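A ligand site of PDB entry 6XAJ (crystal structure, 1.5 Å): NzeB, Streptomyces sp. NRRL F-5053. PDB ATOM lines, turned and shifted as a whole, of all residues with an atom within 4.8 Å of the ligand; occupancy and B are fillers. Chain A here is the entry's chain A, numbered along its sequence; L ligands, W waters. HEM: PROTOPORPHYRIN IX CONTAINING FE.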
ATOM      1  N   SER A  64      11.084 -17.908   3.372  1.00  0.00           N
ATOM      2  CA  SER A  64      12.486 -18.042   3.722  1.00  0.00           C
ATOM      3  C   SER A  64      13.363 -17.494   2.608  1.00  0.00           C
ATOM      4  O   SER A  64      14.326 -16.755   2.856  1.00  0.00           O
ATOM      5  CB  SER A  64      12.807 -19.520   3.973  1.00  0.00           C
ATOM      6  OG  SER A  64      14.204 -19.710   4.116  1.00  0.00           O
ATOM      7  N   ILE A  90      18.678 -23.695  -3.341  1.00  0.00           N
ATOM      8  CA  ILE A  90      17.471 -24.509  -3.309  1.00  0.00           C
ATOM      9  C   ILE A  90      16.585 -24.225  -4.508  1.00  0.00           C
ATOM     10  O   ILE A  90      16.053 -25.141  -5.149  1.00  0.00           O
ATOM     11  CB  ILE A  90      16.741 -24.359  -1.971  1.00  0.00           C
ATOM     12  CG1 ILE A  90      17.552 -25.004  -0.832  1.00  0.00           C
ATOM     13  CG2 ILE A  90      15.349 -24.991  -2.041  1.00  0.00           C
ATOM     14  CD1 ILE A  90      17.246 -24.435   0.534  1.00  0.00           C
ATOM     15  N   LEU A 102      17.207 -32.949  -2.918  1.00  0.00           N
ATOM     16  CA  LEU A 102      17.738 -32.721  -1.574  1.00  0.00           C
ATOM     17  C   LEU A 102      17.174 -33.746  -0.599  1.00  0.00           C
ATOM     18  O   LEU A 102      17.916 -34.583  -0.069  1.00  0.00           O
ATOM     19  CB  LEU A 102      17.411 -31.312  -1.096  1.00  0.00           C
ATOM     20  CG  LEU A 102      18.293 -30.170  -1.619  1.00  0.00           C
ATOM     21  CD1 LEU A 102      18.186 -28.942  -0.737  1.00  0.00           C
ATOM     22  CD2 LEU A 102      19.741 -30.630  -1.732  1.00  0.00           C
ATOM     23  N   LEU A 106      18.504 -37.881   0.994  1.00  0.00           N
ATOM     24  CA  LEU A 106      18.750 -37.886   2.439  1.00  0.00           C
ATOM     25  C   LEU A 106      17.653 -38.619   3.200  1.00  0.00           C
ATOM     26  O   LEU A 106      17.615 -38.565   4.429  1.00  0.00           O
ATOM     27  CB  LEU A 106      18.853 -36.452   2.949  1.00  0.00           C
ATOM     28  CG  LEU A 106      19.893 -35.522   2.299  1.00  0.00           C
ATOM     29  CD1 LEU A 106      19.515 -34.063   2.509  1.00  0.00           C
ATOM     30  CD2 LEU A 106      21.258 -35.782   2.909  1.00  0.00           C
ATOM     31  N   LEU A 150      30.908 -38.243   7.572  1.00  0.00           N
ATOM     32  CA  LEU A 150      29.535 -38.008   7.144  1.00  0.00           C
ATOM     33  C   LEU A 150      29.493 -37.101   5.928  1.00  0.00           C
ATOM     34  O   LEU A 150      28.794 -37.383   4.946  1.00  0.00           O
ATOM     35  CB  LEU A 150      28.720 -37.418   8.301  1.00  0.00           C
ATOM     36  CG  LEU A 150      27.236 -37.166   8.029  1.00  0.00           C
ATOM     37  CD1 LEU A 150      26.491 -38.500   8.041  1.00  0.00           C
ATOM     38  CD2 LEU A 150      26.639 -36.236   9.062  1.00  0.00           C
ATOM     39  N   LEU A 155      27.557 -36.402   1.444  1.00  0.00           N
ATOM     40  CA  LEU A 155      27.249 -35.104   0.847  1.00  0.00           C
ATOM     41  C   LEU A 155      28.116 -34.761  -0.359  1.00  0.00           C
ATOM     42  O   LEU A 155      27.603 -34.478  -1.436  1.00  0.00           O
ATOM     43  CB  LEU A 155      27.297 -33.981   1.885  1.00  0.00           C
ATOM     44  CG  LEU A 155      26.398 -34.163   3.117  1.00  0.00           C
ATOM     45  CD1 LEU A 155      26.473 -32.952   4.038  1.00  0.00           C
ATOM     46  CD2 LEU A 155      24.956 -34.443   2.702  1.00  0.00           C
ATOM     47  N   LEU A 211      25.434 -36.969  -2.132  1.00  0.00           N
ATOM     48  CA  LEU A 211      24.355 -36.118  -2.614  1.00  0.00           C
ATOM     49  C   LEU A 211      24.794 -35.291  -3.827  1.00  0.00           C
ATOM     50  O   LEU A 211      24.006 -35.105  -4.764  1.00  0.00           O
ATOM     51  CB  LEU A 211      23.868 -35.219  -1.484  1.00  0.00           C
ATOM     52  CG  LEU A 211      22.585 -34.430  -1.736  1.00  0.00           C
ATOM     53  CD1 LEU A 211      21.476 -35.340  -2.245  1.00  0.00           C
ATOM     54  CD2 LEU A 211      22.159 -33.700  -0.468  1.00  0.00           C
ATOM     55  N   LEU A 236      26.006 -24.886  -0.343  1.00  0.00           N
ATOM     56  CA  LEU A 236      24.847 -25.124   0.514  1.00  0.00           C
ATOM     57  C   LEU A 236      25.057 -26.346   1.401  1.00  0.00           C
ATOM     58  O   LEU A 236      24.751 -26.309   2.593  1.00  0.00           O
ATOM     59  CB  LEU A 236      23.590 -25.311  -0.335  1.00  0.00           C
ATOM     60  CG  LEU A 236      22.372 -25.798   0.461  1.00  0.00           C
ATOM     61  CD1 LEU A 236      21.903 -24.746   1.458  1.00  0.00           C
ATOM     62  CD2 LEU A 236      21.234 -26.181  -0.477  1.00  0.00           C
ATOM     63  N   LEU A 237      25.581 -27.437   0.832  1.00  0.00           N
ATOM     64  CA  LEU A 237      25.769 -28.649   1.617  1.00  0.00           C
ATOM     65  C   LEU A 237      26.812 -28.454   2.719  1.00  0.00           C
ATOM     66  O   LEU A 237      26.666 -28.998   3.817  1.00  0.00           O
ATOM     67  CB  LEU A 237      26.127 -29.826   0.708  1.00  0.00           C
ATOM     68  CG  LEU A 237      25.049 -30.204  -0.319  1.00  0.00           C
ATOM     69  CD1 LEU A 237      25.454 -31.441  -1.111  1.00  0.00           C
ATOM     70  CD2 LEU A 237      23.676 -30.394   0.346  1.00  0.00           C
ATOM     71  N   ALA A 240      25.061 -26.097   5.367  1.00  0.00           N
ATOM     72  CA  ALA A 240      23.929 -26.728   6.048  1.00  0.00           C
ATOM     73  C   ALA A 240      24.328 -27.969   6.843  1.00  0.00           C
ATOM     74  O   ALA A 240      23.680 -28.296   7.845  1.00  0.00           O
ATOM     75  CB  ALA A 240      22.857 -27.119   5.023  1.00  0.00           C
ATOM     76  N   GLY A 241      25.375 -28.676   6.418  1.00  0.00           N
ATOM     77  CA  GLY A 241      25.674 -29.975   6.984  1.00  0.00           C
ATOM     78  C   GLY A 241      26.923 -30.060   7.836  1.00  0.00           C
ATOM     79  O   GLY A 241      27.035 -30.956   8.672  1.00  0.00           O
ATOM     80  N   THR A 244      26.730 -27.529  11.524  1.00  0.00           N
ATOM     81  CA  THR A 244      25.596 -27.995  12.291  1.00  0.00           C
ATOM     82  C   THR A 244      25.890 -29.362  12.903  1.00  0.00           C
ATOM     83  O   THR A 244      25.701 -29.576  14.101  1.00  0.00           O
ATOM     84  CB  THR A 244      24.425 -28.134  11.341  1.00  0.00           C
ATOM     85  OG1 THR A 244      24.894 -28.838  10.183  1.00  0.00           O
ATOM     86  CG2 THR A 244      23.899 -26.756  10.941  1.00  0.00           C
ATOM     87  N   SER A 245      26.366 -30.297  12.087  1.00  0.00           N
ATOM     88  CA  SER A 245      26.658 -31.629  12.595  1.00  0.00           C
ATOM     89  C   SER A 245      27.772 -31.580  13.632  1.00  0.00           C
ATOM     90  O   SER A 245      27.678 -32.230  14.681  1.00  0.00           O
ATOM     91  CB  SER A 245      26.997 -32.564  11.443  1.00  0.00           C
ATOM     92  OG  SER A 245      25.909 -32.664  10.542  1.00  0.00           O
ATOM     93  N   PHE A 248      26.464 -29.660  16.825  1.00  0.00           N
ATOM     94  CA  PHE A 248      25.455 -30.379  17.598  1.00  0.00           C
ATOM     95  C   PHE A 248      26.035 -31.605  18.288  1.00  0.00           C
ATOM     96  O   PHE A 248      25.704 -31.902  19.438  1.00  0.00           O
ATOM     97  CB  PHE A 248      24.241 -30.781  16.760  1.00  0.00           C
ATOM     98  CG  PHE A 248      23.144 -31.337  17.616  1.00  0.00           C
ATOM     99  CD1 PHE A 248      22.283 -30.472  18.295  1.00  0.00           C
ATOM    100  CD2 PHE A 248      23.043 -32.694  17.843  1.00  0.00           C
ATOM    101  CE1 PHE A 248      21.332 -30.973  19.132  1.00  0.00           C
ATOM    102  CE2 PHE A 248      22.082 -33.191  18.698  1.00  0.00           C
ATOM    103  CZ  PHE A 248      21.216 -32.316  19.336  1.00  0.00           C
ATOM    104  N   LEU A 281      17.893 -33.043  20.907  1.00  0.00           N
ATOM    105  CA  LEU A 281      17.566 -32.033  19.904  1.00  0.00           C
ATOM    106  C   LEU A 281      16.754 -30.886  20.479  1.00  0.00           C
ATOM    107  O   LEU A 281      16.878 -29.756  20.012  1.00  0.00           O
ATOM    108  CB  LEU A 281      16.840 -32.711  18.744  1.00  0.00           C
ATOM    109  CG  LEU A 281      17.794 -33.498  17.841  1.00  0.00           C
ATOM    110  CD1 LEU A 281      17.050 -34.594  17.089  1.00  0.00           C
ATOM    111  CD2 LEU A 281      18.539 -32.566  16.869  1.00  0.00           C
ATOM    112  N   LEU A 286      21.895 -25.051  19.704  1.00  0.00           N
ATOM    113  CA  LEU A 286      22.837 -25.066  18.582  1.00  0.00           C
ATOM    114  C   LEU A 286      23.078 -23.664  18.045  1.00  0.00           C
ATOM    115  O   LEU A 286      24.162 -23.107  18.252  1.00  0.00           O
ATOM    116  CB  LEU A 286      22.379 -26.032  17.486  1.00  0.00           C
ATOM    117  CG  LEU A 286      23.383 -26.124  16.332  1.00  0.00           C
ATOM    118  CD1 LEU A 286      24.766 -26.634  16.815  1.00  0.00           C
ATOM    119  CD2 LEU A 286      22.814 -27.009  15.256  1.00  0.00           C
ATOM    120  N   VAL A 291      16.250 -18.592  12.894  1.00  0.00           N
ATOM    121  CA  VAL A 291      15.783 -18.761  11.517  1.00  0.00           C
ATOM    122  C   VAL A 291      14.958 -17.543  11.152  1.00  0.00           C
ATOM    123  O   VAL A 291      14.441 -16.844  12.028  1.00  0.00           O
ATOM    124  CB  VAL A 291      15.013 -20.082  11.307  1.00  0.00           C
ATOM    125  CG1 VAL A 291      15.879 -21.301  11.693  1.00  0.00           C
ATOM    126  CG2 VAL A 291      13.722 -20.101  12.079  1.00  0.00           C
ATOM    127  N   ARG A 293      12.269 -15.302   8.235  1.00  0.00           N
ATOM    128  CA  ARG A 293      11.299 -15.308   7.149  1.00  0.00           C
ATOM    129  C   ARG A 293      10.881 -13.874   6.858  1.00  0.00           C
ATOM    130  O   ARG A 293      10.793 -13.053   7.777  1.00  0.00           O
ATOM    131  CB  ARG A 293      10.010 -16.092   7.496  1.00  0.00           C
ATOM    132  CG  ARG A 293      10.204 -17.580   7.875  1.00  0.00           C
ATOM    133  CD  ARG A 293      10.623 -18.408   6.686  1.00  0.00           C
ATOM    134  NE  ARG A 293      10.674 -19.830   7.013  1.00  0.00           N
ATOM    135  CZ  ARG A 293      11.764 -20.466   7.446  1.00  0.00           C
ATOM    136  NH1 ARG A 293      12.913 -19.817   7.618  1.00  0.00           N
ATOM    137  NH2 ARG A 293      11.694 -21.757   7.708  1.00  0.00           N
ATOM    138  N   LEU A 316      15.036 -20.907  17.647  1.00  0.00           N
ATOM    139  CA  LEU A 316      14.661 -22.283  17.927  1.00  0.00           C
ATOM    140  C   LEU A 316      14.998 -22.681  19.349  1.00  0.00           C
ATOM    141  O   LEU A 316      14.256 -23.450  19.974  1.00  0.00           O
ATOM    142  CB  LEU A 316      15.337 -23.226  16.927  1.00  0.00           C
ATOM    143  CG  LEU A 316      15.162 -22.824  15.460  1.00  0.00           C
ATOM    144  CD1 LEU A 316      15.988 -23.764  14.605  1.00  0.00           C
ATOM    145  CD2 LEU A 316      13.702 -22.844  15.042  1.00  0.00           C
ATOM    146  N   PHE A 342      11.749 -28.096  18.000  1.00  0.00           N
ATOM    147  CA  PHE A 342      12.075 -27.245  16.861  1.00  0.00           C
ATOM    148  C   PHE A 342      13.537 -27.340  16.466  1.00  0.00           C
ATOM    149  O   PHE A 342      14.032 -26.474  15.743  1.00  0.00           O
ATOM    150  CB  PHE A 342      11.753 -25.786  17.194  1.00  0.00           C
ATOM    151  CG  PHE A 342      10.345 -25.352  16.859  1.00  0.00           C
ATOM    152  CD1 PHE A 342       9.263 -25.862  17.551  1.00  0.00           C
ATOM    153  CD2 PHE A 342      10.131 -24.411  15.875  1.00  0.00           C
ATOM    154  CE1 PHE A 342       7.968 -25.432  17.249  1.00  0.00           C
ATOM    155  CE2 PHE A 342       8.849 -23.976  15.563  1.00  0.00           C
ATOM    156  CZ  PHE A 342       7.767 -24.486  16.255  1.00  0.00           C
ATOM    157  N   GLY A 343      14.236 -28.382  16.912  1.00  0.00           N
ATOM    158  CA  GLY A 343      15.651 -28.508  16.598  1.00  0.00           C
ATOM    159  C   GLY A 343      15.935 -28.570  15.106  1.00  0.00           C
ATOM    160  O   GLY A 343      17.052 -28.255  14.663  1.00  0.00           O
ATOM    161  N   PHE A 344      14.975 -29.055  14.324  1.00  0.00           N
ATOM    162  CA  PHE A 344      15.099 -29.113  12.877  1.00  0.00           C
ATOM    163  C   PHE A 344      14.179 -28.109  12.195  1.00  0.00           C
ATOM    164  O   PHE A 344      13.937 -28.235  10.993  1.00  0.00           O
ATOM    165  CB  PHE A 344      14.745 -30.515  12.355  1.00  0.00           C
ATOM    166  CG  PHE A 344      15.751 -31.573  12.712  1.00  0.00           C
ATOM    167  CD1 PHE A 344      17.097 -31.400  12.390  1.00  0.00           C
ATOM    168  CD2 PHE A 344      15.353 -32.735  13.334  1.00  0.00           C
ATOM    169  CE1 PHE A 344      18.023 -32.390  12.719  1.00  0.00           C
ATOM    170  CE2 PHE A 344      16.265 -33.732  13.652  1.00  0.00           C
ATOM    171  CZ  PHE A 344      17.612 -33.558  13.340  1.00  0.00           C
ATOM    172  N   GLY A 345      13.646 -27.140  12.926  1.00  0.00           N
ATOM    173  CA  GLY A 345      12.704 -26.219  12.322  1.00  0.00           C
ATOM    174  C   GLY A 345      11.295 -26.799  12.296  1.00  0.00           C
ATOM    175  O   GLY A 345      10.926 -27.649  13.112  1.00  0.00           O
ATOM    176  N   ARG A 348       7.567 -26.106   5.845  1.00  0.00           N
ATOM    177  CA  ARG A 348       8.079 -26.373   4.499  1.00  0.00           C
ATOM    178  C   ARG A 348       9.587 -26.600   4.519  1.00  0.00           C
ATOM    179  O   ARG A 348      10.100 -27.447   3.767  1.00  0.00           O
ATOM    180  CB  ARG A 348       7.735 -25.214   3.573  1.00  0.00           C
ATOM    181  CG  ARG A 348       8.596 -25.149   2.320  1.00  0.00           C
ATOM    182  CD  ARG A 348       8.225 -23.967   1.430  1.00  0.00           C
ATOM    183  NE  ARG A 348       6.841 -24.048   0.980  1.00  0.00           N
ATOM    184  CZ  ARG A 348       6.453 -24.659  -0.144  1.00  0.00           C
ATOM    185  NH1 ARG A 348       7.353 -25.238  -0.928  1.00  0.00           N
ATOM    186  NH2 ARG A 348       5.176 -24.682  -0.476  1.00  0.00           N
ATOM    187  N   HIS A 349      10.302 -25.858   5.361  1.00  0.00           N
ATOM    188  CA  HIS A 349      11.755 -25.879   5.341  1.00  0.00           C
ATOM    189  C   HIS A 349      12.360 -26.732   6.450  1.00  0.00           C
ATOM    190  O   HIS A 349      13.547 -26.574   6.746  1.00  0.00           O
ATOM    191  CB  HIS A 349      12.316 -24.456   5.385  1.00  0.00           C
ATOM    192  CG  HIS A 349      11.828 -23.604   4.249  1.00  0.00           C
ATOM    193  ND1 HIS A 349      12.404 -23.631   3.005  1.00  0.00           N
ATOM    194  CD2 HIS A 349      10.830 -22.685   4.186  1.00  0.00           C
ATOM    195  CE1 HIS A 349      11.776 -22.789   2.207  1.00  0.00           C
ATOM    196  NE2 HIS A 349      10.821 -22.198   2.897  1.00  0.00           N
ATOM    197  N   PHE A 350      11.559 -27.620   7.044  1.00  0.00           N
ATOM    198  CA  PHE A 350      12.072 -28.624   7.983  1.00  0.00           C
ATOM    199  C   PHE A 350      13.325 -29.275   7.418  1.00  0.00           C
ATOM    200  O   PHE A 350      13.357 -29.651   6.247  1.00  0.00           O
ATOM    201  CB  PHE A 350      10.988 -29.701   8.182  1.00  0.00           C
ATOM    202  CG  PHE A 350      11.215 -30.599   9.363  1.00  0.00           C
ATOM    203  CD1 PHE A 350      10.866 -30.201  10.653  1.00  0.00           C
ATOM    204  CD2 PHE A 350      11.798 -31.848   9.201  1.00  0.00           C
ATOM    205  CE1 PHE A 350      11.068 -31.034  11.737  1.00  0.00           C
ATOM    206  CE2 PHE A 350      11.987 -32.688  10.286  1.00  0.00           C
ATOM    207  CZ  PHE A 350      11.645 -32.273  11.554  1.00  0.00           C
ATOM    208  N   CYS A 351      14.354 -29.392   8.256  1.00  0.00           N
ATOM    209  CA  CYS A 351      15.668 -29.813   7.794  1.00  0.00           C
ATOM    210  C   CYS A 351      15.571 -31.103   6.970  1.00  0.00           C
ATOM    211  O   CYS A 351      15.194 -32.152   7.512  1.00  0.00           O
ATOM    212  CB  CYS A 351      16.557 -30.056   9.000  1.00  0.00           C
ATOM    213  SG  CYS A 351      18.200 -30.696   8.518  1.00  0.00           S
ATOM    214  N   PRO A 352      15.927 -31.069   5.683  1.00  0.00           N
ATOM    215  CA  PRO A 352      15.935 -32.318   4.910  1.00  0.00           C
ATOM    216  C   PRO A 352      17.035 -33.275   5.341  1.00  0.00           C
ATOM    217  O   PRO A 352      16.968 -34.474   5.023  1.00  0.00           O
ATOM    218  CB  PRO A 352      16.163 -31.850   3.460  1.00  0.00           C
ATOM    219  CG  PRO A 352      16.868 -30.544   3.599  1.00  0.00           C
ATOM    220  CD  PRO A 352      16.344 -29.918   4.873  1.00  0.00           C
ATOM    221  N   GLY A 353      18.047 -32.803   6.056  1.00  0.00           N
ATOM    222  CA  GLY A 353      19.066 -33.657   6.637  1.00  0.00           C
ATOM    223  C   GLY A 353      18.659 -34.308   7.947  1.00  0.00           C
ATOM    224  O   GLY A 353      19.486 -34.964   8.594  1.00  0.00           O
ATOM    225  N   LEU A 356      19.358 -38.256   8.477  1.00  0.00           N
ATOM    226  CA  LEU A 356      20.790 -38.503   8.586  1.00  0.00           C
ATOM    227  C   LEU A 356      21.355 -37.960   9.903  1.00  0.00           C
ATOM    228  O   LEU A 356      22.186 -38.608  10.540  1.00  0.00           O
ATOM    229  CB  LEU A 356      21.493 -37.860   7.398  1.00  0.00           C
ATOM    230  CG  LEU A 356      22.957 -38.193   7.215  1.00  0.00           C
ATOM    231  CD1 LEU A 356      23.120 -39.712   7.072  1.00  0.00           C
ATOM    232  CD2 LEU A 356      23.462 -37.453   5.991  1.00  0.00           C
ATOM    233  N   ALA A 357      20.945 -36.752  10.296  1.00  0.00           N
ATOM    234  CA  ALA A 357      21.408 -36.177  11.556  1.00  0.00           C
ATOM    235  C   ALA A 357      20.976 -37.052  12.734  1.00  0.00           C
ATOM    236  O   ALA A 357      21.791 -37.391  13.604  1.00  0.00           O
ATOM    237  CB  ALA A 357      20.886 -34.748  11.705  1.00  0.00           C
ATOM    238  N   ILE A 361      23.475 -38.802  15.411  1.00  0.00           N
ATOM    239  CA  ILE A 361      23.293 -38.545  16.839  1.00  0.00           C
ATOM    240  C   ILE A 361      23.029 -39.849  17.587  1.00  0.00           C
ATOM    241  O   ILE A 361      23.612 -40.115  18.654  1.00  0.00           O
ATOM    242  CB  ILE A 361      22.153 -37.524  17.073  1.00  0.00           C
ATOM    243  CG1 ILE A 361      22.498 -36.176  16.433  1.00  0.00           C
ATOM    244  CG2 ILE A 361      21.949 -37.352  18.547  1.00  0.00           C
ATOM    245  CD1 ILE A 361      21.238 -35.339  16.077  1.00  0.00           C
HETATM  246  CHA HEM L   1      17.428 -26.647   7.172  1.00  0.00           C
HETATM  247  CHB HEM L   1      18.996 -28.009  11.602  1.00  0.00           C
HETATM  248  CHC HEM L   1      22.054 -31.166   9.600  1.00  0.00           C
HETATM  249  CHD HEM L   1      20.573 -29.790   5.202  1.00  0.00           C
HETATM  250  C1A HEM L   1      17.559 -26.757   8.542  1.00  0.00           C
HETATM  251  C2A HEM L   1      16.810 -26.033   9.539  1.00  0.00           C
HETATM  252  C3A HEM L   1      17.253 -26.409  10.741  1.00  0.00           C
HETATM  253  C4A HEM L   1      18.309 -27.388  10.561  1.00  0.00           C
HETATM  254  CMA HEM L   1      16.791 -25.925  12.110  1.00  0.00           C
HETATM  255  CAA HEM L   1      15.661 -25.003   9.290  1.00  0.00           C
HETATM  256  CBA HEM L   1      16.161 -23.678   8.758  1.00  0.00           C
HETATM  257  CGA HEM L   1      15.002 -22.740   8.507  1.00  0.00           C
HETATM  258  O1A HEM L   1      13.866 -23.016   8.965  1.00  0.00           O
HETATM  259  O2A HEM L   1      15.274 -21.707   7.852  1.00  0.00           O
HETATM  260  C1B HEM L   1      19.965 -28.985  11.469  1.00  0.00           C
HETATM  261  C2B HEM L   1      20.639 -29.673  12.546  1.00  0.00           C
HETATM  262  C3B HEM L   1      21.513 -30.545  11.969  1.00  0.00           C
HETATM  263  C4B HEM L   1      21.377 -30.429  10.538  1.00  0.00           C
HETATM  264  CMB HEM L   1      20.410 -29.417  14.043  1.00  0.00           C
HETATM  265  CAB HEM L   1      22.497 -31.552  12.612  1.00  0.00           C
HETATM  266  CBB HEM L   1      22.478 -31.903  13.898  1.00  0.00           C
HETATM  267  C1C HEM L   1      21.891 -31.119   8.245  1.00  0.00           C
HETATM  268  C2C HEM L   1      22.566 -31.963   7.277  1.00  0.00           C
HETATM  269  C3C HEM L   1      22.155 -31.588   6.065  1.00  0.00           C
HETATM  270  C4C HEM L   1      21.218 -30.483   6.208  1.00  0.00           C
HETATM  271  CMC HEM L   1      23.557 -33.103   7.611  1.00  0.00           C
HETATM  272  CAC HEM L   1      22.640 -32.246   4.743  1.00  0.00           C
HETATM  273  CBC HEM L   1      22.114 -31.957   3.555  1.00  0.00           C
HETATM  274  C1D HEM L   1      19.652 -28.766   5.333  1.00  0.00           C
HETATM  275  C2D HEM L   1      19.089 -27.935   4.267  1.00  0.00           C
HETATM  276  C3D HEM L   1      18.232 -27.081   4.816  1.00  0.00           C
HETATM  277  C4D HEM L   1      18.200 -27.321   6.243  1.00  0.00           C
HETATM  278  CMD HEM L   1      19.449 -28.056   2.773  1.00  0.00           C
HETATM  279  CAD HEM L   1      17.406 -25.998   4.081  1.00  0.00           C
HETATM  280  CBD HEM L   1      15.987 -26.498   3.807  1.00  0.00           C
HETATM  281  CGD HEM L   1      15.160 -25.393   3.211  1.00  0.00           C
HETATM  282  O1D HEM L   1      15.489 -24.186   3.417  1.00  0.00           O
HETATM  283  O2D HEM L   1      14.159 -25.728   2.534  1.00  0.00           O
HETATM  284  NA  HEM L   1      18.477 -27.580   9.207  1.00  0.00           N
HETATM  285  NB  HEM L   1      20.428 -29.469  10.261  1.00  0.00           N
HETATM  286  NC  HEM L   1      21.078 -30.237   7.558  1.00  0.00           N
HETATM  287  ND  HEM L   1      19.092 -28.356   6.524  1.00  0.00           N
HETATM  288 FE   HEM L   1      19.706 -29.004   8.419  1.00  0.00          FE
HETATM  289  O   HOH W   1      14.861 -21.873   4.950  1.00  0.00           O
HETATM  290  O   HOH W   2      21.171 -27.404   8.307  1.00  0.00           O
HETATM  291  O   HOH W   3      16.362 -19.221   8.232  1.00  0.00           O
HETATM  292  O   HOH W   4      12.183 -25.000   9.315  1.00  0.00           O
HETATM  293  O   HOH W   5      14.922 -21.847   1.415  1.00  0.00           O
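The backbone carbonyl oxygen (O) of Ala 240 lies close to a nitrogen (NC) of the ligand, at 3.3 Å. CD1 of Ile 90 touches O1D of the ligand (3.4 Å). CD1 of Leu 102 touches CMD of the ligand (3.8 Å). CD1 of Leu 106 touches CBC of the ligand, at 3.5 Å. CD2 of Leu 155 touches CAC of the ligand, at 3.8 Å. Leu 237 touches the ligand (CD2 to CBC, 3.9 Å). Gly 241 touches the ligand (CA to C2C, 3.7 Å). OG1 of Thr 244 touches CHC of the ligand, 3.7 Å away. Ser 245 touches the ligand (OG to CMC, 3.8 Å). Phe 248 touches the ligand. Leu 286 touches the ligand (CD2 to CMB, 3.6 Å). CG1 of Val 291 touches CGA of the ligand, at 3.6 Å. CD1 of Leu 316 touches CMA of the ligand, at 3.4 Å. Gly 343 touches the ligand (O to CMA, 3.5 Å). Phe 344 touches the ligand. N of Gly 345 touches CMA of the ligand (3.5 Å). Pro 352 touches the ligand. CA of Gly 353 touches C3C of the ligand, 3.8 Å away. Ala 357 touches the ligand. Hydrophobic or aromatic side chains that line the ligand: Ile 90, Leu 102, Leu 106, Leu 155, Leu 237, Ala 240, Phe 248, Leu 286, Val 291, Leu 316, Phe 344, His 349, Pro 352 and Ala 357. Within 4 Å of the ligand: Ile 90, Leu 102, Leu 106, Leu 155, Leu 237, Ala 240, Gly 241, Thr 244, Ser 245, Phe 248, Leu 286, Val 291, Arg 293, Leu 316, Gly 343, Phe 344, Gly 345, His 349, Cys 351, Pro 352, Gly 353 and Ala 357. The nearest printed residue that does not touch the ligand is Leu 236 (4.2 Å).
The side-chain sulfur (SG) of Cys 351 is bound to an iron atom (FE) of the ligand, at 2.3 Å. O2D of the ligand is in hydrogen-bond range of ND1 of His 349. The guanidinium group of Arg 293 is in salt-bridge range of an oxygen (O1A) of the ligand (2.8 Å).
Water W4 bridges O1A of the ligand (2.6 Å) and O of His 349 (3.3 Å). Water W1 lies within hydrogen-bond range of OG of Ser 64 (2.4 Å) and O1D of the ligand (2.8 Å). Water W5 bridges an oxygen (O1D) of the ligand (3.1 Å) and a ring nitrogen (ND1) of His 349 (3.5 Å).
The backbone NH of Cys 351 sits at hydrogen-bond distance from the backbone carbonyl oxygen of Phe 344 (3.0 Å). The side-chain sulfur of Cys 351 lies close to the backbone NH of Gly 353 (3.2 Å). OG1 of Thr 244 sits at hydrogen-bond distance from O of Ala 240 (2.7 Å). The backbone carbonyl oxygen of Gly 241 sits close to the side-chain hydroxyl of Thr 244, 3.4 Å away. OG of Ser 245 is in hydrogen-bond range of O of Gly 241, at 2.8 Å. The backbone carbonyl oxygen (O) of Leu 155 is in hydrogen-bond range of the backbone NH (N) of Leu 211 (3.4 Å).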
